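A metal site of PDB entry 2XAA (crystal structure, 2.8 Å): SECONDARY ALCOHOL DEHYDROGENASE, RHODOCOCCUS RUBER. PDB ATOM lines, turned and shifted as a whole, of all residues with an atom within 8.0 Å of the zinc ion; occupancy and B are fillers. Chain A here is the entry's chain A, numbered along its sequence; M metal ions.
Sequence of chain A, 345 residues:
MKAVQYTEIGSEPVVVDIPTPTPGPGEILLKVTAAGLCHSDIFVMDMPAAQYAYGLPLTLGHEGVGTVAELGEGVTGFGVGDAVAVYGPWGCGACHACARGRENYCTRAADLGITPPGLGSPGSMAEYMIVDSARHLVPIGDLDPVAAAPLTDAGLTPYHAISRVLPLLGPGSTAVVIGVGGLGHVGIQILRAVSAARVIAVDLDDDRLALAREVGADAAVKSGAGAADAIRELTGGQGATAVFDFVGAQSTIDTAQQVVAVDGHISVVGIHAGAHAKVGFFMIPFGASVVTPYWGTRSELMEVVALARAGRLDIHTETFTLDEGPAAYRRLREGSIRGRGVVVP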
ATOM      1  N   TRP A  90      18.128  -4.160  17.025  1.00  0.00           N
ATOM      2  CA  TRP A  90      18.900  -4.192  15.772  1.00  0.00           C
ATOM      3  C   TRP A  90      19.343  -5.588  15.398  1.00  0.00           C
ATOM      4  O   TRP A  90      19.725  -6.383  16.256  1.00  0.00           O
ATOM      5  CB  TRP A  90      20.163  -3.334  15.873  1.00  0.00           C
ATOM      6  CG  TRP A  90      19.931  -1.880  16.221  1.00  0.00           C
ATOM      7  CD1 TRP A  90      18.740  -1.194  16.189  1.00  0.00           C
ATOM      8  CD2 TRP A  90      20.920  -0.935  16.624  1.00  0.00           C
ATOM      9  NE1 TRP A  90      18.928   0.104  16.563  1.00  0.00           N
ATOM     10  CE2 TRP A  90      20.256   0.291  16.831  1.00  0.00           C
ATOM     11  CE3 TRP A  90      22.295  -1.011  16.853  1.00  0.00           C
ATOM     12  CZ2 TRP A  90      20.938   1.452  17.255  1.00  0.00           C
ATOM     13  CZ3 TRP A  90      22.977   0.150  17.277  1.00  0.00           C
ATOM     14  CH2 TRP A  90      22.291   1.351  17.468  1.00  0.00           C
ATOM     15  N   GLY A  91      19.291  -5.864  14.105  1.00  0.00           N
ATOM     16  CA  GLY A  91      19.754  -7.122  13.557  1.00  0.00           C
ATOM     17  C   GLY A  91      20.502  -6.933  12.255  1.00  0.00           C
ATOM     18  O   GLY A  91      20.701  -5.797  11.815  1.00  0.00           O
ATOM     19  N   CYS A  92      20.873  -8.032  11.608  1.00  0.00           N
ATOM     20  CA  CYS A  92      21.751  -8.001  10.445  1.00  0.00           C
ATOM     21  C   CYS A  92      21.220  -7.181   9.259  1.00  0.00           C
ATOM     22  O   CYS A  92      21.988  -6.575   8.530  1.00  0.00           O
ATOM     23  CB  CYS A  92      22.083  -9.421  10.031  1.00  0.00           C
ATOM     24  SG  CYS A  92      20.767 -10.207   9.180  1.00  0.00           S
ATOM     25  N   GLY A  93      19.891  -7.145   9.090  1.00  0.00           N
ATOM     26  CA  GLY A  93      19.228  -6.389   8.004  1.00  0.00           C
ATOM     27  C   GLY A  93      19.116  -7.152   6.695  1.00  0.00           C
ATOM     28  O   GLY A  93      18.542  -6.663   5.703  1.00  0.00           O
ATOM     29  N   ALA A  94      19.625  -8.384   6.721  1.00  0.00           N
ATOM     30  CA  ALA A  94      19.855  -9.155   5.515  1.00  0.00           C
ATOM     31  C   ALA A  94      19.318 -10.602   5.550  1.00  0.00           C
ATOM     32  O   ALA A  94      19.306 -11.252   4.504  1.00  0.00           O
ATOM     33  CB  ALA A  94      21.363  -9.111   5.134  1.00  0.00           C
ATOM     34  N   CYS A  95      18.871 -11.112   6.701  1.00  0.00           N
ATOM     35  CA  CYS A  95      18.258 -12.461   6.722  1.00  0.00           C
ATOM     36  C   CYS A  95      16.816 -12.424   6.227  1.00  0.00           C
ATOM     37  O   CYS A  95      16.289 -11.369   5.844  1.00  0.00           O
ATOM     38  CB  CYS A  95      18.367 -13.136   8.097  1.00  0.00           C
ATOM     39  SG  CYS A  95      17.669 -12.208   9.519  1.00  0.00           S
ATOM     40  N   HIS A  96      16.156 -13.580   6.236  1.00  0.00           N
ATOM     41  CA  HIS A  96      14.763 -13.652   5.820  1.00  0.00           C
ATOM     42  C   HIS A  96      13.866 -12.778   6.725  1.00  0.00           C
ATOM     43  O   HIS A  96      12.982 -12.039   6.238  1.00  0.00           O
ATOM     44  CB  HIS A  96      14.280 -15.092   5.777  1.00  0.00           C
ATOM     45  CG  HIS A  96      12.906 -15.245   5.218  1.00  0.00           C
ATOM     46  ND1 HIS A  96      11.822 -15.628   5.987  1.00  0.00           N
ATOM     47  CD2 HIS A  96      12.419 -15.026   3.965  1.00  0.00           C
ATOM     48  CE1 HIS A  96      10.742 -15.656   5.235  1.00  0.00           C
ATOM     49  NE2 HIS A  96      11.070 -15.296   4.006  1.00  0.00           N
ATOM     50  N   ALA A  97      14.127 -12.840   8.036  1.00  0.00           N
ATOM     51  CA  ALA A  97      13.362 -12.060   9.002  1.00  0.00           C
ATOM     52  C   ALA A  97      13.609 -10.537   8.847  1.00  0.00           C
ATOM     53  O   ALA A  97      12.666  -9.727   8.832  1.00  0.00           O
ATOM     54  CB  ALA A  97      13.688 -12.528  10.410  1.00  0.00           C
ATOM     55  N   CYS A  98      14.879 -10.185   8.706  1.00  0.00           N
ATOM     56  CA  CYS A  98      15.299  -8.794   8.684  1.00  0.00           C
ATOM     57  C   CYS A  98      14.800  -8.098   7.417  1.00  0.00           C
ATOM     58  O   CYS A  98      14.494  -6.903   7.441  1.00  0.00           O
ATOM     59  CB  CYS A  98      16.820  -8.698   8.793  1.00  0.00           C
ATOM     60  SG  CYS A  98      17.600  -8.805  10.447  1.00  0.00           S
ATOM     61  N   ALA A  99      14.713  -8.847   6.326  1.00  0.00           N
ATOM     62  CA  ALA A  99      14.225  -8.300   5.061  1.00  0.00           C
ATOM     63  C   ALA A  99      12.775  -7.913   5.151  1.00  0.00           C
ATOM     64  O   ALA A  99      12.331  -7.012   4.448  1.00  0.00           O
ATOM     65  CB  ALA A  99      14.424  -9.304   3.934  1.00  0.00           C
ATOM     66  N   ARG A 102      11.603  -7.608  10.315  1.00  0.00           N
ATOM     67  CA  ARG A 102      11.311  -8.296  11.579  1.00  0.00           C
ATOM     68  C   ARG A 102      12.583  -8.471  12.445  1.00  0.00           C
ATOM     69  O   ARG A 102      12.884  -9.579  12.940  1.00  0.00           O
ATOM     70  CB  ARG A 102      10.643  -9.655  11.322  1.00  0.00           C
ATOM     71  CG  ARG A 102       9.401  -9.587  10.503  1.00  0.00           C
ATOM     72  CD  ARG A 102       8.934 -10.990  10.204  1.00  0.00           C
ATOM     73  NE  ARG A 102       8.277 -11.671  11.317  1.00  0.00           N
ATOM     74  CZ  ARG A 102       7.079 -11.333  11.810  1.00  0.00           C
ATOM     75  NH1 ARG A 102       6.424 -10.291  11.296  1.00  0.00           N
ATOM     76  NH2 ARG A 102       6.562 -12.020  12.830  1.00  0.00           N
ATOM     77  N   GLU A 103      13.331  -7.380  12.638  1.00  0.00           N
ATOM     78  CA  GLU A 103      14.695  -7.543  13.104  1.00  0.00           C
ATOM     79  C   GLU A 103      14.765  -8.097  14.527  1.00  0.00           C
ATOM     80  O   GLU A 103      15.757  -8.724  14.927  1.00  0.00           O
ATOM     81  CB  GLU A 103      15.506  -6.265  12.901  1.00  0.00           C
ATOM     82  CG  GLU A 103      15.560  -5.842  11.444  1.00  0.00           C
ATOM     83  CD  GLU A 103      16.618  -4.806  11.164  1.00  0.00           C
ATOM     84  OE1 GLU A 103      17.572  -4.733  11.938  1.00  0.00           O
ATOM     85  OE2 GLU A 103      16.530  -4.089  10.159  1.00  0.00           O
ATOM     86  N   ASN A 104      13.657  -7.914  15.251  1.00  0.00           N
ATOM     87  CA  ASN A 104      13.483  -8.520  16.570  1.00  0.00           C
ATOM     88  C   ASN A 104      13.624 -10.048  16.563  1.00  0.00           C
ATOM     89  O   ASN A 104      13.963 -10.648  17.580  1.00  0.00           O
ATOM     90  CB  ASN A 104      12.144  -8.102  17.185  1.00  0.00           C
ATOM     91  CG  ASN A 104      10.952  -8.449  16.295  1.00  0.00           C
ATOM     92  OD1 ASN A 104      11.055  -8.408  15.065  1.00  0.00           O
ATOM     93  ND2 ASN A 104       9.802  -8.773  16.918  1.00  0.00           N
ATOM     94  N   TYR A 105      13.404 -10.668  15.403  1.00  0.00           N
ATOM     95  CA  TYR A 105      13.553 -12.119  15.273  1.00  0.00           C
ATOM     96  C   TYR A 105      14.718 -12.479  14.326  1.00  0.00           C
ATOM     97  O   TYR A 105      14.711 -13.556  13.706  1.00  0.00           O
ATOM     98  CB  TYR A 105      12.227 -12.767  14.806  1.00  0.00           C
ATOM     99  CG  TYR A 105      11.035 -12.618  15.741  1.00  0.00           C
ATOM    100  CD1 TYR A 105      11.116 -13.014  17.078  1.00  0.00           C
ATOM    101  CD2 TYR A 105       9.834 -12.070  15.292  1.00  0.00           C
ATOM    102  CE1 TYR A 105      10.049 -12.863  17.951  1.00  0.00           C
ATOM    103  CE2 TYR A 105       8.737 -11.931  16.161  1.00  0.00           C
ATOM    104  CZ  TYR A 105       8.853 -12.336  17.498  1.00  0.00           C
ATOM    105  OH  TYR A 105       7.795 -12.240  18.393  1.00  0.00           O
ATOM    106  N   CYS A 106      15.707 -11.580  14.206  1.00  0.00           N
ATOM    107  CA  CYS A 106      16.879 -11.787  13.365  1.00  0.00           C
ATOM    108  C   CYS A 106      17.692 -12.980  13.823  1.00  0.00           C
ATOM    109  O   CYS A 106      17.965 -13.130  15.011  1.00  0.00           O
ATOM    110  CB  CYS A 106      17.786 -10.560  13.421  1.00  0.00           C
ATOM    111  SG  CYS A 106      19.347 -10.881  12.637  1.00  0.00           S
ATOM    112  N   THR A 107      18.112 -13.806  12.885  1.00  0.00           N
ATOM    113  CA  THR A 107      18.789 -15.060  13.247  1.00  0.00           C
ATOM    114  C   THR A 107      20.284 -14.895  13.443  1.00  0.00           C
ATOM    115  O   THR A 107      20.933 -15.735  14.079  1.00  0.00           O
ATOM    116  CB  THR A 107      18.561 -16.159  12.178  1.00  0.00           C
ATOM    117  OG1 THR A 107      18.901 -15.645  10.888  1.00  0.00           O
ATOM    118  CG2 THR A 107      17.078 -16.635  12.168  1.00  0.00           C
ATOM    119  N   ARG A 108      20.845 -13.826  12.900  1.00  0.00           N
ATOM    120  CA  ARG A 108      22.289 -13.708  12.797  1.00  0.00           C
ATOM    121  C   ARG A 108      22.915 -12.710  13.796  1.00  0.00           C
ATOM    122  O   ARG A 108      24.146 -12.645  13.950  1.00  0.00           O
ATOM    123  CB  ARG A 108      22.644 -13.319  11.364  1.00  0.00           C
ATOM    124  CG  ARG A 108      22.385 -14.394  10.280  1.00  0.00           C
ATOM    125  CD  ARG A 108      23.554 -15.399  10.045  1.00  0.00           C
ATOM    126  NE  ARG A 108      24.910 -14.934  10.431  1.00  0.00           N
ATOM    127  CZ  ARG A 108      25.591 -15.383  11.491  1.00  0.00           C
ATOM    128  NH1 ARG A 108      26.801 -14.894  11.775  1.00  0.00           N
ATOM    129  NH2 ARG A 108      25.067 -16.319  12.285  1.00  0.00           N
ATOM    130  N   ALA A 109      22.081 -11.955  14.494  1.00  0.00           N
ATOM    131  CA  ALA A 109      22.585 -10.878  15.338  1.00  0.00           C
ATOM    132  C   ALA A 109      23.425 -11.398  16.515  1.00  0.00           C
ATOM    133  O   ALA A 109      24.555 -10.925  16.734  1.00  0.00           O
ATOM    134  CB  ALA A 109      21.447  -9.997  15.830  1.00  0.00           C
ATOM    135  N   LEU A 112      26.694 -12.379  15.116  1.00  0.00           N
ATOM    136  CA  LEU A 112      27.479 -11.294  14.608  1.00  0.00           C
ATOM    137  C   LEU A 112      27.785 -10.343  15.755  1.00  0.00           C
ATOM    138  O   LEU A 112      28.433  -9.314  15.536  1.00  0.00           O
ATOM    139  CB  LEU A 112      26.732 -10.567  13.471  1.00  0.00           C
ATOM    140  CG  LEU A 112      26.694 -11.090  12.031  1.00  0.00           C
ATOM    141  CD1 LEU A 112      25.594 -10.374  11.234  1.00  0.00           C
ATOM    142  CD2 LEU A 112      28.036 -10.961  11.289  1.00  0.00           C
ATOM    143  N   ILE A 114      25.444  -8.343  17.597  1.00  0.00           N
ATOM    144  CA  ILE A 114      24.746  -7.093  17.311  1.00  0.00           C
ATOM    145  C   ILE A 114      23.730  -6.944  18.423  1.00  0.00           C
ATOM    146  O   ILE A 114      22.838  -7.779  18.575  1.00  0.00           O
ATOM    147  CB  ILE A 114      24.104  -7.076  15.906  1.00  0.00           C
ATOM    148  CG1 ILE A 114      25.182  -6.777  14.844  1.00  0.00           C
ATOM    149  CG2 ILE A 114      22.979  -6.058  15.828  1.00  0.00           C
ATOM    150  CD1 ILE A 114      24.637  -6.452  13.408  1.00  0.00           C
ATOM    151  N   ARG A 135      18.248   2.842   8.564  1.00  0.00           N
ATOM    152  CA  ARG A 135      16.973   2.150   8.661  1.00  0.00           C
ATOM    153  C   ARG A 135      16.420   2.103  10.096  1.00  0.00           C
ATOM    154  O   ARG A 135      15.246   1.767  10.293  1.00  0.00           O
ATOM    155  CB  ARG A 135      17.089   0.727   8.084  1.00  0.00           C
ATOM    156  CG  ARG A 135      17.733  -0.319   8.987  1.00  0.00           C
ATOM    157  CD  ARG A 135      18.117  -1.571   8.212  1.00  0.00           C
ATOM    158  NE  ARG A 135      18.638  -2.619   9.093  1.00  0.00           N
ATOM    159  CZ  ARG A 135      19.925  -2.824   9.343  1.00  0.00           C
ATOM    160  NH1 ARG A 135      20.852  -2.064   8.776  1.00  0.00           N
ATOM    161  NH2 ARG A 135      20.304  -3.807  10.175  1.00  0.00           N
HETATM  162 ZN    ZN M   1      18.887 -10.538  10.381  1.00  0.00          ZN
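N of Gly 93 sits close to SG of Cys 98, 3.1 Å away.
The side-chain sulfur of Cys 95 lies close to the backbone NH of Thr 107, at 3.8 Å.
The backbone NH (N) of Ala 94 lies close to the side-chain sulfur (SG) of Cys 92 (3.3 Å).
SG of Cys 106 lies close to N of Arg 108 (3.3 Å).
The side-chain sulfur of Cys 106 lies close to the backbone NH of Ala 109 (3.5 Å).
Merely in contact with the zinc ion: Gly 93.
Five residues have an atom within 4 Å of the zinc ion: Cys 92, Gly 93, Cys 95, Cys 98 and Cys 106.
The zinc ion is bound by SG of Cys 98, at 2.2 Å.
SG of Cys 95 binds the zinc ion, at 2.2 Å.
SG of Cys 92 binds the zinc ion, at 2.3 Å.
The zinc ion is bound by SG of Cys 106 (2.3 Å).
The zinc ion has four donor atoms within binding distance.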
